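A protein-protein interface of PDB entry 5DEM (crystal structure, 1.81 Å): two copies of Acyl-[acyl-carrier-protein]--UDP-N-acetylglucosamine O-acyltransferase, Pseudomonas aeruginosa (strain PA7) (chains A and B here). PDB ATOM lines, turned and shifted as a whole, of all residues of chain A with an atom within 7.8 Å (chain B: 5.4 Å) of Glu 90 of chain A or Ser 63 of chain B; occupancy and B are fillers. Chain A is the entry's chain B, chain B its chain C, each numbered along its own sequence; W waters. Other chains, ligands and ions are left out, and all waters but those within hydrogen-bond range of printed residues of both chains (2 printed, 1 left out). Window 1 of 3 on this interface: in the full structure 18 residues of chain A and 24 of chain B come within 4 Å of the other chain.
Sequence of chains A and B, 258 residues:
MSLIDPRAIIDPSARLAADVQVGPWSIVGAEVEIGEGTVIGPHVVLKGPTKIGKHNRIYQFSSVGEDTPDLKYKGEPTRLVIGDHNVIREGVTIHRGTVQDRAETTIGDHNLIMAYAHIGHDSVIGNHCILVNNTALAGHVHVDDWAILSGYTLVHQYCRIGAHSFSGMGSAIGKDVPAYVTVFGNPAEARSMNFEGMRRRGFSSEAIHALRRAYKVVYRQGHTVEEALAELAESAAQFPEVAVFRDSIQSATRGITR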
ATOM      1  N   ILE A  58      25.839 -16.743  -1.525  1.00  0.00           N
ATOM      2  CA  ILE A  58      25.437 -16.016  -2.724  1.00  0.00           C
ATOM      3  C   ILE A  58      23.989 -16.292  -3.055  1.00  0.00           C
ATOM      4  O   ILE A  58      23.579 -17.453  -3.236  1.00  0.00           O
ATOM      5  CB  ILE A  58      26.328 -16.331  -3.946  1.00  0.00           C
ATOM      6  CG1 ILE A  58      27.791 -16.067  -3.616  1.00  0.00           C
ATOM      7  CG2 ILE A  58      25.860 -15.508  -5.145  1.00  0.00           C
ATOM      8  CD1 ILE A  58      28.755 -16.337  -4.753  1.00  0.00           C
ATOM      9  N   TYR A  59      23.166 -15.241  -3.006  1.00  0.00           N
ATOM     10  CA  TYR A  59      21.739 -15.336  -3.189  1.00  0.00           C
ATOM     11  C   TYR A  59      21.275 -15.359  -4.648  1.00  0.00           C
ATOM     12  O   TYR A  59      21.969 -14.920  -5.568  1.00  0.00           O
ATOM     13  CB  TYR A  59      21.011 -14.193  -2.454  1.00  0.00           C
ATOM     14  CG  TYR A  59      20.893 -14.400  -0.955  1.00  0.00           C
ATOM     15  CD1 TYR A  59      22.005 -14.377  -0.141  1.00  0.00           C
ATOM     16  CD2 TYR A  59      19.647 -14.535  -0.359  1.00  0.00           C
ATOM     17  CE1 TYR A  59      21.906 -14.558   1.227  1.00  0.00           C
ATOM     18  CE2 TYR A  59      19.533 -14.664   1.012  1.00  0.00           C
ATOM     19  CZ  TYR A  59      20.665 -14.756   1.780  1.00  0.00           C
ATOM     20  OH  TYR A  59      20.583 -14.934   3.146  1.00  0.00           O
ATOM     21  N   GLN A  60      20.054 -15.806  -4.813  1.00  0.00           N
ATOM     22  CA  GLN A  60      19.373 -15.886  -6.110  1.00  0.00           C
ATOM     23  C   GLN A  60      19.477 -14.635  -6.982  1.00  0.00           C
ATOM     24  O   GLN A  60      19.402 -13.486  -6.484  1.00  0.00           O
ATOM     25  CB  GLN A  60      17.890 -16.201  -5.925  1.00  0.00           C
ATOM     26  CG  GLN A  60      17.158 -15.265  -4.999  1.00  0.00           C
ATOM     27  CD  GLN A  60      17.098 -15.763  -3.578  1.00  0.00           C
ATOM     28  OE1 GLN A  60      17.995 -16.452  -3.099  1.00  0.00           O
ATOM     29  NE2 GLN A  60      16.127 -15.219  -2.815  1.00  0.00           N
ATOM     30  N   PHE A  61      19.615 -14.895  -8.274  1.00  0.00           N
ATOM     31  CA  PHE A  61      19.478 -13.911  -9.358  1.00  0.00           C
ATOM     32  C   PHE A  61      20.718 -13.042  -9.452  1.00  0.00           C
ATOM     33  O   PHE A  61      20.754 -12.119 -10.254  1.00  0.00           O
ATOM     34  CB  PHE A  61      18.213 -13.031  -9.265  1.00  0.00           C
ATOM     35  CG  PHE A  61      16.939 -13.802  -8.975  1.00  0.00           C
ATOM     36  CD1 PHE A  61      16.559 -14.862  -9.811  1.00  0.00           C
ATOM     37  CD2 PHE A  61      16.139 -13.472  -7.907  1.00  0.00           C
ATOM     38  CE1 PHE A  61      15.401 -15.572  -9.575  1.00  0.00           C
ATOM     39  CE2 PHE A  61      14.930 -14.162  -7.680  1.00  0.00           C
ATOM     40  CZ  PHE A  61      14.581 -15.217  -8.515  1.00  0.00           C
ATOM     41  N   SER A  62      21.755 -13.418  -8.724  1.00  0.00           N
ATOM     42  CA  SER A  62      23.053 -12.802  -8.861  1.00  0.00           C
ATOM     43  C   SER A  62      23.790 -13.318 -10.087  1.00  0.00           C
ATOM     44  O   SER A  62      23.642 -14.495 -10.480  1.00  0.00           O
ATOM     45  CB  SER A  62      23.866 -13.084  -7.595  1.00  0.00           C
ATOM     46  OG  SER A  62      23.313 -12.367  -6.495  1.00  0.00           O
ATOM     47  N   SER A  63      24.593 -12.450 -10.691  1.00  0.00           N
ATOM     48  CA  SER A  63      25.470 -12.807 -11.804  1.00  0.00           C
ATOM     49  C   SER A  63      26.879 -12.429 -11.408  1.00  0.00           C
ATOM     50  O   SER A  63      27.215 -11.235 -11.361  1.00  0.00           O
ATOM     51  CB  SER A  63      25.121 -12.050 -13.072  1.00  0.00           C
ATOM     52  OG  SER A  63      23.842 -12.394 -13.531  1.00  0.00           O
ATOM     53  N   VAL A  87      28.759 -12.107   2.122  1.00  0.00           N
ATOM     54  CA  VAL A  87      27.393 -12.325   1.822  1.00  0.00           C
ATOM     55  C   VAL A  87      27.026 -11.455   0.630  1.00  0.00           C
ATOM     56  O   VAL A  87      27.226 -10.235   0.677  1.00  0.00           O
ATOM     57  CB  VAL A  87      26.460 -11.994   3.012  1.00  0.00           C
ATOM     58  CG1 VAL A  87      25.000 -12.042   2.605  1.00  0.00           C
ATOM     59  CG2 VAL A  87      26.716 -12.926   4.181  1.00  0.00           C
ATOM     60  N   ILE A  88      26.596 -12.101  -0.452  1.00  0.00           N
ATOM     61  CA  ILE A  88      26.211 -11.434  -1.676  1.00  0.00           C
ATOM     62  C   ILE A  88      24.730 -11.705  -1.844  1.00  0.00           C
ATOM     63  O   ILE A  88      24.302 -12.854  -2.066  1.00  0.00           O
ATOM     64  CB  ILE A  88      27.035 -11.971  -2.853  1.00  0.00           C
ATOM     65  CG1 ILE A  88      28.496 -11.602  -2.664  1.00  0.00           C
ATOM     66  CG2 ILE A  88      26.465 -11.467  -4.188  1.00  0.00           C
ATOM     67  CD1 ILE A  88      29.456 -12.340  -3.555  1.00  0.00           C
ATOM     68  N   ARG A  89      23.920 -10.647  -1.719  1.00  0.00           N
ATOM     69  CA  ARG A  89      22.481 -10.759  -1.747  1.00  0.00           C
ATOM     70  C   ARG A  89      21.848 -10.858  -3.138  1.00  0.00           C
ATOM     71  O   ARG A  89      22.532 -11.053  -4.152  1.00  0.00           O
ATOM     72  CB  ARG A  89      21.854  -9.625  -0.894  1.00  0.00           C
ATOM     73  CG  ARG A  89      22.182  -9.712   0.595  1.00  0.00           C
ATOM     74  CD  ARG A  89      21.548 -10.906   1.314  1.00  0.00           C
ATOM     75  NE  ARG A  89      20.108 -10.918   1.175  1.00  0.00           N
ATOM     76  CZ  ARG A  89      19.235 -11.186   2.148  1.00  0.00           C
ATOM     77  NH1 ARG A  89      19.641 -11.468   3.372  1.00  0.00           N
ATOM     78  NH2 ARG A  89      17.952 -11.139   1.877  1.00  0.00           N
ATOM     79  N   GLU A  90      20.529 -10.725  -3.201  1.00  0.00           N
ATOM     80  CA  GLU A  90      19.773 -10.937  -4.422  1.00  0.00           C
ATOM     81  C   GLU A  90      20.154 -10.005  -5.560  1.00  0.00           C
ATOM     82  O   GLU A  90      20.233  -8.778  -5.364  1.00  0.00           O
ATOM     83  CB  GLU A  90      18.273 -10.756  -4.156  1.00  0.00           C
ATOM     84  CG  GLU A  90      17.696 -11.513  -2.947  1.00  0.00           C
ATOM     85  CD  GLU A  90      17.621 -10.693  -1.670  1.00  0.00           C
ATOM     86  OE1 GLU A  90      18.659 -10.093  -1.269  1.00  0.00           O
ATOM     87  OE2 GLU A  90      16.591 -10.796  -0.935  1.00  0.00           O
ATOM     88  N   GLY A  91      20.339 -10.559  -6.753  1.00  0.00           N
ATOM     89  CA  GLY A  91      20.501  -9.765  -7.945  1.00  0.00           C
ATOM     90  C   GLY A  91      21.771  -8.945  -8.054  1.00  0.00           C
ATOM     91  O   GLY A  91      21.864  -8.073  -8.885  1.00  0.00           O
ATOM     92  N   VAL A  92      22.778  -9.286  -7.271  1.00  0.00           N
ATOM     93  CA  VAL A  92      24.053  -8.562  -7.340  1.00  0.00           C
ATOM     94  C   VAL A  92      24.771  -8.939  -8.630  1.00  0.00           C
ATOM     95  O   VAL A  92      24.725 -10.098  -9.064  1.00  0.00           O
ATOM     96  CB  VAL A  92      24.908  -8.888  -6.113  1.00  0.00           C
ATOM     97  CG1 VAL A  92      26.350  -8.415  -6.281  1.00  0.00           C
ATOM     98  CG2 VAL A  92      24.274  -8.290  -4.856  1.00  0.00           C
ATOM     99  N   THR A  93      25.391  -7.960  -9.274  1.00  0.00           N
ATOM    100  CA  THR A  93      26.223  -8.182 -10.466  1.00  0.00           C
ATOM    101  C   THR A  93      27.684  -7.819 -10.164  1.00  0.00           C
ATOM    102  O   THR A  93      27.962  -6.787  -9.525  1.00  0.00           O
ATOM    103  CB  THR A  93      25.754  -7.396 -11.700  1.00  0.00           C
ATOM    104  OG1 THR A  93      25.690  -5.999 -11.398  1.00  0.00           O
ATOM    105  CG2 THR A  93      24.395  -7.898 -12.155  1.00  0.00           C
ATOM    106  N   ILE A 113      27.237  -7.394   0.688  1.00  0.00           N
ATOM    107  CA  ILE A 113      26.871  -6.706  -0.552  1.00  0.00           C
ATOM    108  C   ILE A 113      25.413  -6.962  -0.762  1.00  0.00           C
ATOM    109  O   ILE A 113      24.991  -8.101  -1.082  1.00  0.00           O
ATOM    110  CB  ILE A 113      27.739  -7.212  -1.707  1.00  0.00           C
ATOM    111  CG1 ILE A 113      29.216  -6.959  -1.386  1.00  0.00           C
ATOM    112  CG2 ILE A 113      27.343  -6.543  -3.016  1.00  0.00           C
ATOM    113  CD1 ILE A 113      30.174  -7.707  -2.282  1.00  0.00           C
ATOM    114  N   MET A 114      24.595  -5.940  -0.528  1.00  0.00           N
ATOM    115  CA  MET A 114      23.160  -6.097  -0.566  1.00  0.00           C
ATOM    116  C   MET A 114      22.513  -6.107  -1.945  1.00  0.00           C
ATOM    117  O   MET A 114      23.174  -5.876  -2.961  1.00  0.00           O
ATOM    118  CB  MET A 114      22.504  -5.055   0.385  1.00  0.00           C
ATOM    119  CG  MET A 114      22.969  -5.164   1.814  1.00  0.00           C
ATOM    120  SD  MET A 114      22.038  -4.054   2.872  1.00  0.00           S
ATOM    121  CE  MET A 114      22.921  -4.166   4.392  1.00  0.00           C
ATOM    122  N   ALA A 115      21.200  -6.294  -1.976  1.00  0.00           N
ATOM    123  CA  ALA A 115      20.498  -6.546  -3.231  1.00  0.00           C
ATOM    124  C   ALA A 115      20.734  -5.528  -4.346  1.00  0.00           C
ATOM    125  O   ALA A 115      20.717  -4.306  -4.132  1.00  0.00           O
ATOM    126  CB  ALA A 115      19.015  -6.705  -2.999  1.00  0.00           C
ATOM    127  N   TYR A 116      21.038  -6.049  -5.536  1.00  0.00           N
ATOM    128  CA  TYR A 116      21.156  -5.266  -6.758  1.00  0.00           C
ATOM    129  C   TYR A 116      22.323  -4.288  -6.745  1.00  0.00           C
ATOM    130  O   TYR A 116      22.466  -3.502  -7.669  1.00  0.00           O
ATOM    131  CB  TYR A 116      19.852  -4.523  -7.120  1.00  0.00           C
ATOM    132  CG  TYR A 116      18.719  -5.478  -7.364  1.00  0.00           C
ATOM    133  CD1 TYR A 116      18.710  -6.318  -8.468  1.00  0.00           C
ATOM    134  CD2 TYR A 116      17.723  -5.636  -6.421  1.00  0.00           C
ATOM    135  CE1 TYR A 116      17.757  -7.336  -8.583  1.00  0.00           C
ATOM    136  CE2 TYR A 116      16.762  -6.630  -6.541  1.00  0.00           C
ATOM    137  CZ  TYR A 116      16.747  -7.442  -7.643  1.00  0.00           C
ATOM    138  OH  TYR A 116      15.736  -8.384  -7.793  1.00  0.00           O
ATOM    139  N   ALA A 117      23.223  -4.465  -5.797  1.00  0.00           N
ATOM    140  CA  ALA A 117      24.497  -3.795  -5.916  1.00  0.00           C
ATOM    141  C   ALA A 117      25.227  -4.218  -7.171  1.00  0.00           C
ATOM    142  O   ALA A 117      25.059  -5.349  -7.677  1.00  0.00           O
ATOM    143  CB  ALA A 117      25.324  -4.046  -4.702  1.00  0.00           C
ATOM    144  N   ASN A 133      21.768  -1.795  -0.667  1.00  0.00           N
ATOM    145  CA  ASN A 133      21.021  -2.030  -1.938  1.00  0.00           C
ATOM    146  C   ASN A 133      21.358  -1.046  -3.047  1.00  0.00           C
ATOM    147  O   ASN A 133      21.280   0.164  -2.818  1.00  0.00           O
ATOM    148  CB  ASN A 133      19.514  -1.869  -1.709  1.00  0.00           C
ATOM    149  CG  ASN A 133      18.937  -2.898  -0.763  1.00  0.00           C
ATOM    150  OD1 ASN A 133      19.498  -3.162   0.300  1.00  0.00           O
ATOM    151  ND2 ASN A 133      17.807  -3.490  -1.151  1.00  0.00           N
ATOM    152  N   ASN A 134      21.625  -1.552  -4.233  1.00  0.00           N
ATOM    153  CA  ASN A 134      21.759  -0.755  -5.444  1.00  0.00           C
ATOM    154  C   ASN A 134      22.940   0.229  -5.409  1.00  0.00           C
ATOM    155  O   ASN A 134      22.974   1.119  -6.200  1.00  0.00           O
ATOM    156  CB  ASN A 134      20.465   0.010  -5.767  1.00  0.00           C
ATOM    157  CG  ASN A 134      19.354  -0.923  -6.212  1.00  0.00           C
ATOM    158  OD1 ASN A 134      18.658  -1.501  -5.384  1.00  0.00           O
ATOM    159  ND2 ASN A 134      19.180  -1.036  -7.497  1.00  0.00           N
ATOM    160  N   VAL B  45      11.027 -16.567  -5.920  1.00  0.00           N
ATOM    161  CA  VAL B  45      11.425 -17.199  -4.673  1.00  0.00           C
ATOM    162  C   VAL B  45      10.562 -16.664  -3.527  1.00  0.00           C
ATOM    163  O   VAL B  45      10.539 -15.442  -3.253  1.00  0.00           O
ATOM    164  CB  VAL B  45      12.906 -17.001  -4.353  1.00  0.00           C
ATOM    165  CG1 VAL B  45      13.300 -17.591  -2.999  1.00  0.00           C
ATOM    166  CG2 VAL B  45      13.764 -17.586  -5.463  1.00  0.00           C
ATOM    167  N   PHE B  61      11.484 -13.172 -10.903  1.00  0.00           N
ATOM    168  CA  PHE B  61      12.743 -12.688 -10.307  1.00  0.00           C
ATOM    169  C   PHE B  61      12.545 -11.917  -8.985  1.00  0.00           C
ATOM    170  O   PHE B  61      13.495 -11.397  -8.434  1.00  0.00           O
ATOM    171  CB  PHE B  61      13.580 -11.893 -11.307  1.00  0.00           C
ATOM    172  CG  PHE B  61      13.686 -12.536 -12.685  1.00  0.00           C
ATOM    173  CD1 PHE B  61      14.176 -13.825 -12.827  1.00  0.00           C
ATOM    174  CD2 PHE B  61      13.274 -11.860 -13.806  1.00  0.00           C
ATOM    175  CE1 PHE B  61      14.239 -14.421 -14.071  1.00  0.00           C
ATOM    176  CE2 PHE B  61      13.409 -12.416 -15.065  1.00  0.00           C
ATOM    177  CZ  PHE B  61      13.771 -13.759 -15.180  1.00  0.00           C
ATOM    178  N   SER B  62      11.341 -11.999  -8.428  1.00  0.00           N
ATOM    179  CA  SER B  62      11.039 -11.415  -7.122  1.00  0.00           C
ATOM    180  C   SER B  62      11.457 -12.376  -6.023  1.00  0.00           C
ATOM    181  O   SER B  62      11.462 -13.608  -6.226  1.00  0.00           O
ATOM    182  CB  SER B  62       9.535 -11.130  -7.045  1.00  0.00           C
ATOM    183  OG  SER B  62       9.178 -10.076  -7.901  1.00  0.00           O
ATOM    184  N   SER B  63      11.945 -11.819  -4.918  1.00  0.00           N
ATOM    185  CA  SER B  63      12.278 -12.541  -3.720  1.00  0.00           C
ATOM    186  C   SER B  63      11.390 -11.960  -2.642  1.00  0.00           C
ATOM    187  O   SER B  63      11.621 -10.845  -2.139  1.00  0.00           O
ATOM    188  CB  SER B  63      13.738 -12.349  -3.312  1.00  0.00           C
ATOM    189  OG  SER B  63      14.582 -12.889  -4.314  1.00  0.00           O
ATOM    190  N   VAL B  64      10.448 -12.778  -2.203  1.00  0.00           N
ATOM    191  CA  VAL B  64       9.424 -12.320  -1.264  1.00  0.00           C
ATOM    192  C   VAL B  64       9.502 -13.168  -0.001  1.00  0.00           C
ATOM    193  O   VAL B  64       9.296 -14.381  -0.044  1.00  0.00           O
ATOM    194  CB  VAL B  64       8.052 -12.393  -1.933  1.00  0.00           C
ATOM    195  CG1 VAL B  64       6.928 -12.056  -0.949  1.00  0.00           C
ATOM    196  CG2 VAL B  64       7.986 -11.485  -3.148  1.00  0.00           C
ATOM    197  N   GLY B  65       9.971 -12.571   1.091  1.00  0.00           N
ATOM    198  CA  GLY B  65       9.983 -13.234   2.401  1.00  0.00           C
ATOM    199  C   GLY B  65      11.346 -13.598   2.887  1.00  0.00           C
ATOM    200  O   GLY B  65      11.494 -14.283   3.893  1.00  0.00           O
ATOM    201  N   GLU B  66      12.392 -13.112   2.212  1.00  0.00           N
ATOM    202  CA  GLU B  66      13.728 -13.280   2.728  1.00  0.00           C
ATOM    203  C   GLU B  66      13.974 -12.566   4.076  1.00  0.00           C
ATOM    204  O   GLU B  66      13.272 -11.603   4.418  1.00  0.00           O
ATOM    205  CB  GLU B  66      14.771 -12.829   1.692  1.00  0.00           C
ATOM    206  CG  GLU B  66      14.920 -13.752   0.499  1.00  0.00           C
ATOM    207  CD  GLU B  66      15.511 -15.113   0.837  1.00  0.00           C
ATOM    208  OE1 GLU B  66      16.086 -15.281   1.939  1.00  0.00           O
ATOM    209  OE2 GLU B  66      15.483 -15.986  -0.059  1.00  0.00           O
ATOM    210  N   GLY B  91      11.409  -8.579 -10.092  1.00  0.00           N
ATOM    211  CA  GLY B  91      12.600  -8.328  -9.298  1.00  0.00           C
ATOM    212  C   GLY B  91      12.369  -7.570  -7.992  1.00  0.00           C
ATOM    213  O   GLY B  91      13.320  -7.089  -7.396  1.00  0.00           O
ATOM    214  N   VAL B  92      11.142  -7.571  -7.495  1.00  0.00           N
ATOM    215  CA  VAL B  92      10.846  -6.892  -6.237  1.00  0.00           C
ATOM    216  C   VAL B  92      11.363  -7.717  -5.061  1.00  0.00           C
ATOM    217  O   VAL B  92      11.362  -8.953  -5.112  1.00  0.00           O
ATOM    218  CB  VAL B  92       9.327  -6.663  -6.090  1.00  0.00           C
ATOM    219  CG1 VAL B  92       8.973  -6.262  -4.676  1.00  0.00           C
ATOM    220  CG2 VAL B  92       8.847  -5.632  -7.114  1.00  0.00           C
ATOM    221  N   THR B  93      11.976  -7.043  -4.086  1.00  0.00           N
ATOM    222  CA  THR B  93      12.448  -7.689  -2.884  1.00  0.00           C
ATOM    223  C   THR B  93      11.634  -7.195  -1.665  1.00  0.00           C
ATOM    224  O   THR B  93      11.350  -5.995  -1.540  1.00  0.00           O
ATOM    225  CB  THR B  93      13.927  -7.465  -2.592  1.00  0.00           C
ATOM    226  OG1 THR B  93      14.230  -6.063  -2.525  1.00  0.00           O
ATOM    227  CG2 THR B  93      14.798  -8.153  -3.673  1.00  0.00           C
ATOM    228  N   ILE B  94      11.103  -8.150  -0.910  1.00  0.00           N
ATOM    229  CA  ILE B  94      10.293  -7.845   0.280  1.00  0.00           C
ATOM    230  C   ILE B  94      10.808  -8.687   1.423  1.00  0.00           C
ATOM    231  O   ILE B  94      10.888  -9.914   1.306  1.00  0.00           O
ATOM    232  CB  ILE B  94       8.805  -8.132   0.071  1.00  0.00           C
ATOM    233  CG1 ILE B  94       8.269  -7.415  -1.153  1.00  0.00           C
ATOM    234  CG2 ILE B  94       8.016  -7.728   1.313  1.00  0.00           C
ATOM    235  CD1 ILE B  94       6.834  -7.757  -1.503  1.00  0.00           C
ATOM    236  N   HIS B  95      11.286  -8.034   2.474  1.00  0.00           N
ATOM    237  CA  HIS B  95      11.878  -8.732   3.598  1.00  0.00           C
ATOM    238  C   HIS B  95      10.883  -8.829   4.759  1.00  0.00           C
ATOM    239  O   HIS B  95      10.019  -7.978   4.906  1.00  0.00           O
ATOM    240  CB  HIS B  95      13.137  -8.042   4.063  1.00  0.00           C
ATOM    241  CG  HIS B  95      14.263  -8.141   3.078  1.00  0.00           C
ATOM    242  ND1 HIS B  95      15.344  -7.293   3.099  1.00  0.00           N
ATOM    243  CD2 HIS B  95      14.409  -8.910   1.973  1.00  0.00           C
ATOM    244  CE1 HIS B  95      16.114  -7.535   2.050  1.00  0.00           C
ATOM    245  NE2 HIS B  95      15.584  -8.533   1.369  1.00  0.00           N
HETATM  246  O   HOH W   1      14.810 -10.810  -5.972  1.00  0.00           O
HETATM  247  O   HOH W   2      16.020 -10.328  -9.248  1.00  0.00           O
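Of chain B, only Ser 63 (3.7 Å), Glu 66 (3.7 Å) and His 95 (3.4 Å) come within 4 Å of Glu 90 of chain A.
Of the printed residues of chain B, Tyr 116 of chain A touches Phe 61 (3.8 Å), Gly 91 (2.8 Å) and Thr 93 (3.8 Å).
Printed residues of chain A within 4 Å of Val 45 of chain B: Gln 60 (3.7 Å) and Phe 61 (3.9 Å).
Of the printed residues of chain A, Phe 61 of chain B touches Phe 61 and Tyr 116.
Of chain A, only Gln 60 (3.2 Å), Phe 61 (3.6 Å) and Glu 90 (3.7 Å) come within 4 Å of Ser 63 of chain B.
Of the printed residues of chain A, Glu 66 of chain B touches Tyr 59, Gln 60, Arg 89 and Glu 90.
Val 92 of chain B touches none of the printed residues of chain A.
The nearest residue of chain B that does not touch Glu 90 of chain A is Thr 93 of chain B (4.2 Å).
The nearest printed residue of chain A that does not touch His 95 of chain B is Asn 133 of chain A (5.4 Å).
Of the 12 printed residues of chain B, 8 touch a printed residue of chain A.
Hydrophobic or aromatic side chains of chain A that line the printed part of chain B: Tyr 59, Phe 61 and Tyr 116.
Among the printed residues, 16 pairs touch across the chains.
Among the printed residues, no Asp or Glu carboxylate lies within 4 Å of a Lys or Arg side-chain nitrogen of the other chain.
OG of Ser 62 of chain A sits at hydrogen-bond distance from O of Tyr 59 of chain A (3.0 Å).
The side-chain hydroxyl (OG) of Ser 62 of chain B lies within hydrogen-bond range of the backbone NH (N) of Gly 91 of chain B, at 3.5 Å.
The backbone NH (N) of Ser 63 of chain B lies within hydrogen-bond range of the backbone carbonyl oxygen (O) of Val 92 of chain B (2.9 Å).
The backbone carbonyl oxygen (O) of Ile 113 of chain A is in hydrogen-bond range of the backbone NH (N) of Arg 89 of chain A, 2.8 Å away.
The backbone NH (N) of Val 45 of chain B is in hydrogen-bond range of the backbone carbonyl oxygen (O) of Ser 62 of chain B, 3.0 Å away.
O of Ile 88 of chain A is in hydrogen-bond range of N of Tyr 59 of chain A, at 2.8 Å.
Phe 61 of chain B touches its own counterpart, Phe 61 of chain A.
Phe 61 of chain A touches Ser 62 of chain B, but with the chains exchanged Ser 62 of chain A does not touch Phe 61 of chain B (8.5 Å).
Phe 61 of chain A touches Ser 63 of chain B, but with the chains exchanged Ser 63 of chain A does not touch Phe 61 of chain B (9.8 Å).
Of the 16 pairs that touch across the chains among the printed residues, 1 has its exchanged pair printed and touching as well.
Water W2 bridges the side-chain hydroxyl of Tyr 116 of chain A (2.4 Å) and the backbone carbonyl oxygen of Phe 61 of chain B (2.9 Å).
Water W1 lies within hydrogen-bond range of OG of Ser 63 of chain B (2.7 Å), O of Phe 61 of chain B (2.9 Å) and OH of Tyr 116 of chain A (3.2 Å).
O of Gly 91 of chain B lies within hydrogen-bond range of OH of Tyr 116 of chain A (2.8 Å).
OE2 of Glu 66 of chain B is in hydrogen-bond range of NE2 of Gln 60 of chain A (2.9 Å).
NE2 of Gln 60 of chain A lies within hydrogen-bond range of OG of Ser 63 of chain B (3.2 Å).
A ring nitrogen (NE2) of His 95 of chain B lies within hydrogen-bond range of the side-chain carboxylate (OE2) of Glu 90 of chain A (3.4 Å).
Among the printed residues, pairs that only touch across the chains: Tyr 59 of chain A with Glu 66 of chain B (3.6 Å), Gln 60 of chain A with Val 45 of chain B (3.7 Å), Phe 61 of chain A with Val 45 of chain B (3.9 Å), Phe 61 of chain A with Phe 61 of chain B (3.2 Å), Phe 61 of chain A with Ser 62 of chain B (3.8 Å), Phe 61 of chain A with Ser 63 of chain B (3.6 Å), Arg 89 of chain A with Glu 66 of chain B (3.6 Å), Arg 89 of chain A with His 95 of chain B (3.6 Å), Glu 90 of chain A with Ser 63 of chain B (3.7 Å), Glu 90 of chain A with Glu 66 of chain B (3.7 Å), Tyr 116 of chain A with Phe 61 of chain B (3.8 Å) and Tyr 116 of chain A with Thr 93 of chain B (3.8 Å).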
